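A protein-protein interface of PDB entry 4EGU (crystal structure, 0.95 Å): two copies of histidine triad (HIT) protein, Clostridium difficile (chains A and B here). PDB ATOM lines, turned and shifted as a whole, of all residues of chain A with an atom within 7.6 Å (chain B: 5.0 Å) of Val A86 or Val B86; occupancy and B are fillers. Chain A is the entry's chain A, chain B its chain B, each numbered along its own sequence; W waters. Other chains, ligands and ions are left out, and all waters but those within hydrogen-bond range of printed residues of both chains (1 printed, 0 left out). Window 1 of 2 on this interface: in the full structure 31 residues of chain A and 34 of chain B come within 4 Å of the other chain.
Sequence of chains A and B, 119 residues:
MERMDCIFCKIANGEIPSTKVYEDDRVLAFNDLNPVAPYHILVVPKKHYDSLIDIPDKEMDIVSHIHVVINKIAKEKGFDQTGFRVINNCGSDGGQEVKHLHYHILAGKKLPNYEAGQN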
ATOM      1  N   VAL A  43       7.641  21.645   8.287  1.00  0.00           N
ATOM      2  CA  VAL A  43       7.189  22.948   8.731  1.00  0.00           C
ATOM      3  C   VAL A  43       5.939  23.295   7.944  1.00  0.00           C
ATOM      4  O   VAL A  43       5.974  23.297   6.710  1.00  0.00           O
ATOM      5  CB  VAL A  43       8.266  24.044   8.531  1.00  0.00           C
ATOM      6  CG1 VAL A  43       7.814  25.329   9.184  1.00  0.00           C
ATOM      7  CG2 VAL A  43       9.605  23.603   9.117  1.00  0.00           C
ATOM      8  N   LEU A  52       2.077  24.997  -3.044  1.00  0.00           N
ATOM      9  CA  LEU A  52       2.676  26.295  -3.288  1.00  0.00           C
ATOM     10  C   LEU A  52       1.928  27.114  -4.346  1.00  0.00           C
ATOM     11  O   LEU A  52       1.778  28.328  -4.215  1.00  0.00           O
ATOM     12  CB  LEU A  52       4.149  26.095  -3.681  1.00  0.00           C
ATOM     13  CG  LEU A  52       4.923  27.336  -4.054  1.00  0.00           C
ATOM     14  CD1 LEU A  52       4.970  28.342  -2.941  1.00  0.00           C
ATOM     15  CD2 LEU A  52       6.328  26.925  -4.466  1.00  0.00           C
ATOM     16  N   ILE A  66       7.689  30.834   7.366  1.00  0.00           N
ATOM     17  CA  ILE A  66       8.200  29.483   7.440  1.00  0.00           C
ATOM     18  C   ILE A  66       9.726  29.464   7.433  1.00  0.00           C
ATOM     19  O   ILE A  66      10.338  28.683   8.156  1.00  0.00           O
ATOM     20  CB  ILE A  66       7.588  28.640   6.313  1.00  0.00           C
ATOM     21  CG1 ILE A  66       6.126  28.297   6.658  1.00  0.00           C
ATOM     22  CG2 ILE A  66       8.411  27.400   6.004  1.00  0.00           C
ATOM     23  CD1 ILE A  66       5.346  27.669   5.496  1.00  0.00           C
ATOM     24  N   HIS A  67      10.347  30.303   6.599  1.00  0.00           N
ATOM     25  CA  HIS A  67      11.808  30.348   6.534  1.00  0.00           C
ATOM     26  C   HIS A  67      12.460  30.955   7.783  1.00  0.00           C
ATOM     27  O   HIS A  67      13.530  30.503   8.179  1.00  0.00           O
ATOM     28  CB  HIS A  67      12.274  31.019   5.257  1.00  0.00           C
ATOM     29  CG  HIS A  67      12.197  30.103   4.063  1.00  0.00           C
ATOM     30  ND1 HIS A  67      11.027  29.735   3.445  1.00  0.00           N
ATOM     31  CD2 HIS A  67      13.173  29.420   3.414  1.00  0.00           C
ATOM     32  CE1 HIS A  67      11.308  28.883   2.459  1.00  0.00           C
ATOM     33  NE2 HIS A  67      12.606  28.678   2.416  1.00  0.00           N
ATOM     34  N   ILE A  70      12.416  27.990  10.032  1.00  0.00           N
ATOM     35  CA  ILE A  70      13.477  27.051   9.686  1.00  0.00           C
ATOM     36  C   ILE A  70      14.804  27.512  10.295  1.00  0.00           C
ATOM     37  O   ILE A  70      15.516  26.718  10.912  1.00  0.00           O
ATOM     38  CB  ILE A  70      13.578  26.912   8.150  1.00  0.00           C
ATOM     39  CG1 ILE A  70      12.355  26.174   7.605  1.00  0.00           C
ATOM     40  CG2 ILE A  70      14.887  26.228   7.751  1.00  0.00           C
ATOM     41  CD1 ILE A  70      12.220  26.206   6.093  1.00  0.00           C
ATOM     42  N   ASN A  71      15.147  28.778  10.101  1.00  0.00           N
ATOM     43  CA  ASN A  71      16.414  29.280  10.609  1.00  0.00           C
ATOM     44  C   ASN A  71      16.447  29.258  12.151  1.00  0.00           C
ATOM     45  O   ASN A  71      17.495  28.976  12.737  1.00  0.00           O
ATOM     46  CB  ASN A  71      16.725  30.673  10.095  1.00  0.00           C
ATOM     47  CG  ASN A  71      17.341  30.664   8.719  1.00  0.00           C
ATOM     48  OD1 ASN A  71      17.526  29.614   8.086  1.00  0.00           O
ATOM     49  ND2 ASN A  71      17.693  31.849   8.253  1.00  0.00           N
ATOM     50  N   PHE A  79      22.434  22.911  13.648  1.00  0.00           N
ATOM     51  CA  PHE A  79      22.691  22.633  12.247  1.00  0.00           C
ATOM     52  C   PHE A  79      22.740  23.897  11.389  1.00  0.00           C
ATOM     53  O   PHE A  79      22.957  23.816  10.182  1.00  0.00           O
ATOM     54  CB  PHE A  79      21.807  21.507  11.666  1.00  0.00           C
ATOM     55  CG  PHE A  79      20.320  21.782  11.669  1.00  0.00           C
ATOM     56  CD1 PHE A  79      19.496  21.199  12.621  1.00  0.00           C
ATOM     57  CD2 PHE A  79      19.737  22.548  10.672  1.00  0.00           C
ATOM     58  CE1 PHE A  79      18.128  21.415  12.603  1.00  0.00           C
ATOM     59  CE2 PHE A  79      18.370  22.766  10.651  1.00  0.00           C
ATOM     60  CZ  PHE A  79      17.566  22.200  11.616  1.00  0.00           C
ATOM     61  N   PHE A  84      22.076  22.335   6.017  1.00  0.00           N
ATOM     62  CA  PHE A  84      20.764  21.715   5.936  1.00  0.00           C
ATOM     63  C   PHE A  84      20.195  21.945   4.541  1.00  0.00           C
ATOM     64  O   PHE A  84      20.708  22.763   3.790  1.00  0.00           O
ATOM     65  CB  PHE A  84      19.812  22.249   7.032  1.00  0.00           C
ATOM     66  CG  PHE A  84      19.596  23.737   7.029  1.00  0.00           C
ATOM     67  CD1 PHE A  84      20.459  24.593   7.693  1.00  0.00           C
ATOM     68  CD2 PHE A  84      18.484  24.278   6.401  1.00  0.00           C
ATOM     69  CE1 PHE A  84      20.228  25.951   7.732  1.00  0.00           C
ATOM     70  CE2 PHE A  84      18.244  25.642   6.435  1.00  0.00           C
ATOM     71  CZ  PHE A  84      19.116  26.481   7.101  1.00  0.00           C
ATOM     72  N   ARG A  85      19.124  21.229   4.225  1.00  0.00           N
ATOM     73  CA  ARG A  85      18.432  21.387   2.955  1.00  0.00           C
ATOM     74  C   ARG A  85      16.950  21.624   3.236  1.00  0.00           C
ATOM     75  O   ARG A  85      16.371  21.029   4.153  1.00  0.00           O
ATOM     76  CB  ARG A  85      18.617  20.123   2.095  1.00  0.00           C
ATOM     77  CG  ARG A  85      18.078  20.245   0.684  1.00  0.00           C
ATOM     78  CD  ARG A  85      18.430  19.026  -0.147  1.00  0.00           C
ATOM     79  NE  ARG A  85      19.867  18.920  -0.299  1.00  0.00           N
ATOM     80  CZ  ARG A  85      20.532  17.791  -0.534  1.00  0.00           C
ATOM     81  NH1 ARG A  85      19.884  16.648  -0.682  1.00  0.00           N
ATOM     82  NH2 ARG A  85      21.838  17.816  -0.560  1.00  0.00           N
ATOM     83  N   VAL A  86      16.374  22.506   2.425  1.00  0.00           N
ATOM     84  CA  VAL A  86      14.950  22.843   2.496  1.00  0.00           C
ATOM     85  C   VAL A  86      14.305  22.401   1.175  1.00  0.00           C
ATOM     86  O   VAL A  86      14.798  22.742   0.107  1.00  0.00           O
ATOM     87  CB  VAL A  86      14.773  24.341   2.696  1.00  0.00           C
ATOM     88  CG1 VAL A  86      13.299  24.740   2.675  1.00  0.00           C
ATOM     89  CG2 VAL A  86      15.455  24.808   3.975  1.00  0.00           C
ATOM     90  N   ILE A  87      13.210  21.654   1.260  1.00  0.00           N
ATOM     91  CA  ILE A  87      12.536  21.118   0.085  1.00  0.00           C
ATOM     92  C   ILE A  87      11.030  21.381   0.172  1.00  0.00           C
ATOM     93  O   ILE A  87      10.389  21.104   1.191  1.00  0.00           O
ATOM     94  CB  ILE A  87      12.774  19.606  -0.078  1.00  0.00           C
ATOM     95  CG1 ILE A  87      14.266  19.259  -0.020  1.00  0.00           C
ATOM     96  CG2 ILE A  87      12.153  19.140  -1.407  1.00  0.00           C
ATOM     97  CD1 ILE A  87      14.682  18.711   1.316  1.00  0.00           C
ATOM     98  N   ASN A  88      10.470  21.868  -0.937  1.00  0.00           N
ATOM     99  CA  ASN A  88       9.028  21.865  -1.146  1.00  0.00           C
ATOM    100  C   ASN A  88       8.717  21.028  -2.383  1.00  0.00           C
ATOM    101  O   ASN A  88       9.319  21.229  -3.440  1.00  0.00           O
ATOM    102  CB  ASN A  88       8.455  23.278  -1.336  1.00  0.00           C
ATOM    103  CG  ASN A  88       6.953  23.238  -1.544  1.00  0.00           C
ATOM    104  OD1 ASN A  88       6.469  23.253  -2.675  1.00  0.00           O
ATOM    105  ND2 ASN A  88       6.214  23.155  -0.467  1.00  0.00           N
ATOM    106  N   ASN A  89       7.773  20.120  -2.233  1.00  0.00           N
ATOM    107  CA  ASN A  89       7.271  19.292  -3.315  1.00  0.00           C
ATOM    108  C   ASN A  89       5.883  19.788  -3.708  1.00  0.00           C
ATOM    109  O   ASN A  89       4.975  19.819  -2.884  1.00  0.00           O
ATOM    110  CB  ASN A  89       7.164  17.844  -2.827  1.00  0.00           C
ATOM    111  CG  ASN A  89       8.497  17.235  -2.474  1.00  0.00           C
ATOM    112  OD1 ASN A  89       9.533  17.578  -3.037  1.00  0.00           O
ATOM    113  ND2 ASN A  89       8.483  16.330  -1.515  1.00  0.00           N
ATOM    114  N   CYS A  90       5.728  20.169  -4.975  1.00  0.00           N
ATOM    115  CA  CYS A  90       4.484  20.756  -5.445  1.00  0.00           C
ATOM    116  C   CYS A  90       3.864  19.899  -6.542  1.00  0.00           C
ATOM    117  O   CYS A  90       4.391  19.781  -7.635  1.00  0.00           O
ATOM    118  CB  CYS A  90       4.735  22.171  -5.967  1.00  0.00           C
ATOM    119  SG  CYS A  90       3.195  23.042  -6.402  1.00  0.00           S
ATOM    120  N   GLY A  94       6.283  16.744  -8.645  1.00  0.00           N
ATOM    121  CA  GLY A  94       7.178  17.193  -7.606  1.00  0.00           C
ATOM    122  C   GLY A  94       7.301  16.168  -6.501  1.00  0.00           C
ATOM    123  O   GLY A  94       8.116  16.338  -5.601  1.00  0.00           O
ATOM    124  N   HIS A 102       3.793  22.318   2.938  1.00  0.00           N
ATOM    125  CA  HIS A 102       4.795  21.938   3.920  1.00  0.00           C
ATOM    126  C   HIS A 102       6.172  22.048   3.324  1.00  0.00           C
ATOM    127  O   HIS A 102       6.365  21.810   2.134  1.00  0.00           O
ATOM    128  CB  HIS A 102       4.556  20.458   4.398  1.00  0.00           C
ATOM    129  CG  HIS A 102       4.598  19.431   3.301  1.00  0.00           C
ATOM    130  ND1 HIS A 102       3.485  19.152   2.556  1.00  0.00           N
ATOM    131  CD2 HIS A 102       5.578  18.613   2.834  1.00  0.00           C
ATOM    132  CE1 HIS A 102       3.768  18.218   1.659  1.00  0.00           C
ATOM    133  NE2 HIS A 102       5.031  17.866   1.814  1.00  0.00           N
ATOM    134  N   TYR A 103       7.129  22.357   4.178  1.00  0.00           N
ATOM    135  CA  TYR A 103       8.528  22.350   3.829  1.00  0.00           C
ATOM    136  C   TYR A 103       9.228  21.283   4.641  1.00  0.00           C
ATOM    137  O   TYR A 103       9.022  21.166   5.839  1.00  0.00           O
ATOM    138  CB  TYR A 103       9.168  23.728   4.092  1.00  0.00           C
ATOM    139  CG  TYR A 103       8.788  24.723   3.030  1.00  0.00           C
ATOM    140  CD1 TYR A 103       7.515  25.251   2.933  1.00  0.00           C
ATOM    141  CD2 TYR A 103       9.696  25.072   2.048  1.00  0.00           C
ATOM    142  CE1 TYR A 103       7.182  26.131   1.892  1.00  0.00           C
ATOM    143  CE2 TYR A 103       9.376  25.954   1.012  1.00  0.00           C
ATOM    144  CZ  TYR A 103       8.121  26.469   0.944  1.00  0.00           C
ATOM    145  OH  TYR A 103       7.766  27.306  -0.078  1.00  0.00           O
ATOM    146  N   HIS A 104      10.078  20.522   3.973  1.00  0.00           N
ATOM    147  CA  HIS A 104      10.971  19.577   4.628  1.00  0.00           C
ATOM    148  C   HIS A 104      12.283  20.268   4.963  1.00  0.00           C
ATOM    149  O   HIS A 104      12.864  20.933   4.102  1.00  0.00           O
ATOM    150  CB  HIS A 104      11.314  18.419   3.692  1.00  0.00           C
ATOM    151  CG  HIS A 104      10.165  17.598   3.220  1.00  0.00           C
ATOM    152  ND1 HIS A 104       9.870  16.375   3.781  1.00  0.00           N
ATOM    153  CD2 HIS A 104       9.319  17.776   2.165  1.00  0.00           C
ATOM    154  CE1 HIS A 104       8.839  15.869   3.125  1.00  0.00           C
ATOM    155  NE2 HIS A 104       8.492  16.688   2.140  1.00  0.00           N
ATOM    156  N   ILE A 105      12.771  20.045   6.188  1.00  0.00           N
ATOM    157  CA  ILE A 105      14.138  20.375   6.561  1.00  0.00           C
ATOM    158  C   ILE A 105      14.873  19.056   6.770  1.00  0.00           C
ATOM    159  O   ILE A 105      14.435  18.231   7.571  1.00  0.00           O
ATOM    160  CB  ILE A 105      14.248  21.157   7.885  1.00  0.00           C
ATOM    161  CG1 ILE A 105      13.274  22.324   8.021  1.00  0.00           C
ATOM    162  CG2 ILE A 105      15.687  21.642   8.066  1.00  0.00           C
ATOM    163  CD1 ILE A 105      13.272  22.906   9.452  1.00  0.00           C
ATOM    164  N   LEU A 106      15.986  18.883   6.055  1.00  0.00           N
ATOM    165  CA  LEU A 106      16.880  17.733   6.255  1.00  0.00           C
ATOM    166  C   LEU A 106      18.193  18.243   6.811  1.00  0.00           C
ATOM    167  O   LEU A 106      18.776  19.177   6.261  1.00  0.00           O
ATOM    168  CB  LEU A 106      17.158  17.008   4.946  1.00  0.00           C
ATOM    169  CG  LEU A 106      15.920  16.486   4.208  1.00  0.00           C
ATOM    170  CD1 LEU A 106      16.362  15.735   2.950  1.00  0.00           C
ATOM    171  CD2 LEU A 106      15.014  15.623   5.037  1.00  0.00           C
ATOM    172  N   LEU A 111      24.315  15.318   3.330  1.00  0.00           N
ATOM    173  CA  LEU A 111      23.204  14.797   2.543  1.00  0.00           C
ATOM    174  C   LEU A 111      23.646  14.424   1.137  1.00  0.00           C
ATOM    175  O   LEU A 111      24.473  15.108   0.546  1.00  0.00           O
ATOM    176  CB  LEU A 111      22.090  15.835   2.454  1.00  0.00           C
ATOM    177  CG  LEU A 111      21.482  16.253   3.780  1.00  0.00           C
ATOM    178  CD1 LEU A 111      20.636  17.502   3.587  1.00  0.00           C
ATOM    179  CD2 LEU A 111      20.646  15.129   4.379  1.00  0.00           C
ATOM    180  N   GLU A 115      18.587  14.071  -6.370  1.00  0.00           N
ATOM    181  CA  GLU A 115      18.080  14.252  -7.729  1.00  0.00           C
ATOM    182  C   GLU A 115      19.159  14.006  -8.772  1.00  0.00           C
ATOM    183  O   GLU A 115      18.847  13.793  -9.934  1.00  0.00           O
ATOM    184  CB  GLU A 115      17.435  15.627  -7.895  1.00  0.00           C
ATOM    185  CG  GLU A 115      16.137  15.787  -7.125  1.00  0.00           C
ATOM    186  CD  GLU A 115      16.307  16.083  -5.651  1.00  0.00           C
ATOM    187  OE1 GLU A 115      15.254  16.084  -5.004  1.00  0.00           O
ATOM    188  OE2 GLU A 115      17.431  16.327  -5.153  1.00  0.00           O
ATOM    189  N   LEU B  52      20.998  30.743   3.043  1.00  0.00           N
ATOM    190  CA  LEU B  52      19.759  30.997   3.744  1.00  0.00           C
ATOM    191  C   LEU B  52      20.000  31.383   5.202  1.00  0.00           C
ATOM    192  O   LEU B  52      19.359  32.278   5.731  1.00  0.00           O
ATOM    193  CB  LEU B  52      18.886  29.734   3.651  1.00  0.00           C
ATOM    194  CG  LEU B  52      17.573  29.698   4.407  1.00  0.00           C
ATOM    195  CD1 LEU B  52      16.684  30.875   4.064  1.00  0.00           C
ATOM    196  CD2 LEU B  52      16.860  28.395   4.122  1.00  0.00           C
ATOM    197  N   HIS B  67       9.547  33.017  -4.230  1.00  0.00           N
ATOM    198  CA  HIS B  67       8.441  32.102  -4.450  1.00  0.00           C
ATOM    199  C   HIS B  67       7.326  32.659  -5.361  1.00  0.00           C
ATOM    200  O   HIS B  67       6.759  31.900  -6.141  1.00  0.00           O
ATOM    201  CB  HIS B  67       7.894  31.593  -3.112  1.00  0.00           C
ATOM    202  CG  HIS B  67       8.761  30.518  -2.476  1.00  0.00           C
ATOM    203  ND1 HIS B  67       9.978  30.753  -1.883  1.00  0.00           N
ATOM    204  CD2 HIS B  67       8.565  29.178  -2.350  1.00  0.00           C
ATOM    205  CE1 HIS B  67      10.484  29.599  -1.447  1.00  0.00           C
ATOM    206  NE2 HIS B  67       9.640  28.629  -1.698  1.00  0.00           N
ATOM    207  N   ILE B  70       8.875  31.912  -8.633  1.00  0.00           N
ATOM    208  CA  ILE B  70       8.785  30.494  -8.944  1.00  0.00           C
ATOM    209  C   ILE B  70       7.405  30.161  -9.527  1.00  0.00           C
ATOM    210  O   ILE B  70       7.299  29.476 -10.548  1.00  0.00           O
ATOM    211  CB  ILE B  70       9.074  29.632  -7.688  1.00  0.00           C
ATOM    212  CG1 ILE B  70      10.552  29.738  -7.315  1.00  0.00           C
ATOM    213  CG2 ILE B  70       8.634  28.194  -7.908  1.00  0.00           C
ATOM    214  CD1 ILE B  70      10.877  29.115  -5.954  1.00  0.00           C
ATOM    215  N   PHE B  84       6.369  20.252  -9.593  1.00  0.00           N
ATOM    216  CA  PHE B  84       7.756  20.660  -9.540  1.00  0.00           C
ATOM    217  C   PHE B  84       8.256  20.582  -8.105  1.00  0.00           C
ATOM    218  O   PHE B  84       7.461  20.474  -7.178  1.00  0.00           O
ATOM    219  CB  PHE B  84       7.951  22.061 -10.137  1.00  0.00           C
ATOM    220  CG  PHE B  84       7.164  23.148  -9.456  1.00  0.00           C
ATOM    221  CD1 PHE B  84       5.859  23.461  -9.866  1.00  0.00           C
ATOM    222  CD2 PHE B  84       7.715  23.892  -8.420  1.00  0.00           C
ATOM    223  CE1 PHE B  84       5.159  24.472  -9.257  1.00  0.00           C
ATOM    224  CE2 PHE B  84       7.009  24.911  -7.822  1.00  0.00           C
ATOM    225  CZ  PHE B  84       5.729  25.197  -8.222  1.00  0.00           C
ATOM    226  N   ARG B  85       9.572  20.651  -7.961  1.00  0.00           N
ATOM    227  CA  ARG B  85      10.232  20.631  -6.652  1.00  0.00           C
ATOM    228  C   ARG B  85      11.087  21.874  -6.506  1.00  0.00           C
ATOM    229  O   ARG B  85      11.740  22.304  -7.454  1.00  0.00           O
ATOM    230  CB  ARG B  85      11.057  19.347  -6.530  1.00  0.00           C
ATOM    231  CG  ARG B  85      11.780  19.179  -5.194  1.00  0.00           C
ATOM    232  CD  ARG B  85      12.406  17.809  -5.046  1.00  0.00           C
ATOM    233  NE  ARG B  85      11.362  16.793  -4.986  1.00  0.00           N
ATOM    234  CZ  ARG B  85      11.529  15.498  -5.209  1.00  0.00           C
ATOM    235  NH1 ARG B  85      12.724  15.014  -5.523  1.00  0.00           N
ATOM    236  NH2 ARG B  85      10.468  14.690  -5.104  1.00  0.00           N
ATOM    237  N   VAL B  86      11.104  22.418  -5.298  1.00  0.00           N
ATOM    238  CA  VAL B  86      11.892  23.605  -4.956  1.00  0.00           C
ATOM    239  C   VAL B  86      12.893  23.191  -3.869  1.00  0.00           C
ATOM    240  O   VAL B  86      12.498  22.612  -2.855  1.00  0.00           O
ATOM    241  CB  VAL B  86      10.966  24.704  -4.415  1.00  0.00           C
ATOM    242  CG1 VAL B  86      11.760  25.906  -3.965  1.00  0.00           C
ATOM    243  CG2 VAL B  86       9.922  25.081  -5.457  1.00  0.00           C
ATOM    244  N   ILE B  87      14.169  23.496  -4.081  1.00  0.00           N
ATOM    245  CA  ILE B  87      15.232  23.103  -3.154  1.00  0.00           C
ATOM    246  C   ILE B  87      16.144  24.268  -2.843  1.00  0.00           C
ATOM    247  O   ILE B  87      16.602  24.974  -3.745  1.00  0.00           O
ATOM    248  CB  ILE B  87      16.096  21.942  -3.731  1.00  0.00           C
ATOM    249  CG1 ILE B  87      15.226  20.718  -4.007  1.00  0.00           C
ATOM    250  CG2 ILE B  87      17.245  21.616  -2.793  1.00  0.00           C
ATOM    251  CD1 ILE B  87      15.939  19.622  -4.766  1.00  0.00           C
ATOM    252  N   ASN B  88      16.463  24.429  -1.553  1.00  0.00           N
ATOM    253  CA  ASN B  88      17.586  25.239  -1.127  1.00  0.00           C
ATOM    254  C   ASN B  88      18.592  24.350  -0.386  1.00  0.00           C
ATOM    255  O   ASN B  88      18.218  23.634   0.539  1.00  0.00           O
ATOM    256  CB  ASN B  88      17.162  26.403  -0.233  1.00  0.00           C
ATOM    257  CG  ASN B  88      18.367  27.226   0.169  1.00  0.00           C
ATOM    258  OD1 ASN B  88      18.997  26.975   1.210  1.00  0.00           O
ATOM    259  ND2 ASN B  88      18.723  28.167  -0.661  1.00  0.00           N
ATOM    260  N   TYR B 103      17.589  29.218  -5.207  1.00  0.00           N
ATOM    261  CA  TYR B 103      16.617  28.145  -5.144  1.00  0.00           C
ATOM    262  C   TYR B 103      16.609  27.397  -6.471  1.00  0.00           C
ATOM    263  O   TYR B 103      16.574  28.004  -7.538  1.00  0.00           O
ATOM    264  CB  TYR B 103      15.228  28.700  -4.808  1.00  0.00           C
ATOM    265  CG  TYR B 103      15.059  28.959  -3.329  1.00  0.00           C
ATOM    266  CD1 TYR B 103      15.720  30.008  -2.706  1.00  0.00           C
ATOM    267  CD2 TYR B 103      14.266  28.135  -2.546  1.00  0.00           C
ATOM    268  CE1 TYR B 103      15.586  30.231  -1.347  1.00  0.00           C
ATOM    269  CE2 TYR B 103      14.125  28.356  -1.189  1.00  0.00           C
ATOM    270  CZ  TYR B 103      14.789  29.404  -0.595  1.00  0.00           C
ATOM    271  OH  TYR B 103      14.665  29.626   0.755  1.00  0.00           O
ATOM    272  N   HIS B 104      16.664  26.074  -6.388  1.00  0.00           N
ATOM    273  CA  HIS B 104      16.531  25.207  -7.534  1.00  0.00           C
ATOM    274  C   HIS B 104      15.046  24.930  -7.766  1.00  0.00           C
ATOM    275  O   HIS B 104      14.345  24.530  -6.830  1.00  0.00           O
ATOM    276  CB  HIS B 104      17.202  23.854  -7.265  1.00  0.00           C
ATOM    277  CG  HIS B 104      18.677  23.894  -6.999  1.00  0.00           C
ATOM    278  ND1 HIS B 104      19.605  23.581  -7.967  1.00  0.00           N
ATOM    279  CD2 HIS B 104      19.375  24.125  -5.856  1.00  0.00           C
ATOM    280  CE1 HIS B 104      20.812  23.666  -7.428  1.00  0.00           C
ATOM    281  NE2 HIS B 104      20.704  23.986  -6.150  1.00  0.00           N
ATOM    282  N   ILE B 105      14.607  25.068  -9.011  1.00  0.00           N
ATOM    283  CA  ILE B 105      13.292  24.612  -9.452  1.00  0.00           C
ATOM    284  C   ILE B 105      13.542  23.444 -10.402  1.00  0.00           C
ATOM    285  O   ILE B 105      14.202  23.616 -11.420  1.00  0.00           O
ATOM    286  CB  ILE B 105      12.470  25.660 -10.229  1.00  0.00           C
ATOM    287  CG1 ILE B 105      12.430  27.048  -9.601  1.00  0.00           C
ATOM    288  CG2 ILE B 105      11.066  25.126 -10.452  1.00  0.00           C
ATOM    289  CD1 ILE B 105      11.786  28.054 -10.576  1.00  0.00           C
HETATM  290  O   HOH W   1      11.640  15.539  -2.037  1.00  0.00           O
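A ring nitrogen (NE2) of His B67 lies within hydrogen-bond range of the side-chain hydroxyl of Tyr A103 (2.8 Å).
The side-chain amide oxygen of Asn A89 sits at hydrogen-bond distance from the guanidinium group of Arg B85, 2.8 Å away.
The backbone carbonyl oxygen of Leu B52 is in hydrogen-bond range of the side-chain amide nitrogen of Asn A71, at 3.1 Å.
The backbone NH (N) of Val A86 sits at hydrogen-bond distance from the backbone carbonyl oxygen (O) of Asn B88 (2.9 Å).
The backbone carbonyl oxygen (O) of Gly A94 is in hydrogen-bond range of the guanidinium group (NH2) of Arg B85, 2.9 Å away.
The backbone NH of Val B86 lies within hydrogen-bond range of the backbone carbonyl oxygen of Asn A88 (2.8 Å).
A ring nitrogen (NE2) of His A67 sits at hydrogen-bond distance from the side-chain hydroxyl of Tyr B103.
OE1 of Glu A115 lies within salt-bridge range of NH1 of Arg B85 (2.8 Å).
O of Phe B84 sits at hydrogen-bond distance from N of Cys A90, at 2.8 Å.
N of Leu A106 sits at hydrogen-bond distance from O of Arg A85 (2.9 Å).
The backbone NH (N) of Val A43 is in hydrogen-bond range of the backbone carbonyl oxygen (O) of Tyr A103 (2.9 Å).
ND2 of Asn A88 is in hydrogen-bond range of O of His A102, 2.9 Å away.
O of Ile B87 sits at hydrogen-bond distance from N of His B104.
O of Ile A87 is in hydrogen-bond range of N of His A104 (2.9 Å).
The backbone carbonyl oxygen (O) of Gly A94 sits close to the side-chain amide oxygen (OD1) of Asn A89, at 3.2 Å.
Phe B84 touches Leu A52 (CE2 to CD2, 3.97 Å).
His A67 touches Leu B52 (CD2 to CD1, 3.9 Å).
Val A86 touches Leu B52 (CG2 to CD2, 3.9 Å).
Val A86 touches Val B86.
Val A86 touches Ile B87.
CG of Arg B85 touches CG2 of Ile A87 (3.8 Å).
Val B86 touches Ile A87.
Phe B84 touches Asn A89 (O to C, 3.9 Å).
Gly A94 touches Phe B84 (CA to O, 3.3 Å).
CD1 of Ile B87 touches OE1 of Glu A115, 3.6 Å away.
Printed residues of chain B within 4 Å of His A67: Leu B52 (3.9 Å) and Tyr B103 (2.8 Å).
Phe A79 touches none of the printed residues of chain B.
Val A86 touches just these residues of chain B: Leu B52 (3.9 Å), Val B86 (3.8 Å), Ile B87 (3.3 Å) and Asn B88 (2.9 Å).
Leu A106 touches none of the printed residues of chain B.
Printed residues of chain A within 4 Å of Phe B84: Leu A52, Asn A89, Cys A90 and Gly A94.
Printed residues of chain A within 4 Å of Arg B85: Ile A87 (3.8 Å), Asn A88 (3.4 Å), Asn A89 (2.8 Å), Gly A94 (2.9 Å) and Glu A115 (2.8 Å).
Val B86 touches just these residues of chain A: Val A86 (3.8 Å), Ile A87 (3.3 Å) and Asn A88 (2.8 Å).
Printed residues of chain A within 4 Å of Tyr B103: His A67.
The nearest residue of chain A that does not touch Val B86 is Leu A52 (4.2 Å).
The nearest printed residue of chain B that does not touch Glu A115 is Val B86 (7.4 Å).
Printed residues of chain B that touch a printed residue of chain A: Leu B52, His B67, Phe B84, Arg B85, Val B86, Ile B87, Asn B88 and Tyr B103.
Of the 22 printed residues of chain A, 13 touch a printed residue of chain B.
Along chain A the printed residues that touch a printed residue of chain B span positions 52 to 115.
Among the printed residues, 24 pairs touch across the chains.
Among the printed residues, Asp or Glu carboxylates within 4 Å of a Lys or Arg side-chain nitrogen of the other chain: Glu A115 with Arg B85.
Arg A85 touches Ile B87, and with the chains exchanged Ile A87 touches Arg B85.
Arg A85 touches Asn B88, and with the chains exchanged Asn A88 touches Arg B85.
Val A86 touches Leu B52, but with the chains exchanged Leu A52 does not touch Val B86 (4.2 Å).
Val A86 touches Ile B87, and with the chains exchanged Ile A87 touches Val B86.
Positions printed for both chains: 52, 67, 70, 84, 85, 86, 87, 88, 103, 104 and 105.
Water W1 lies within hydrogen-bond range of OD1 of Asn A89 (3.1 Å) and NE of Arg B85 (3.2 Å).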
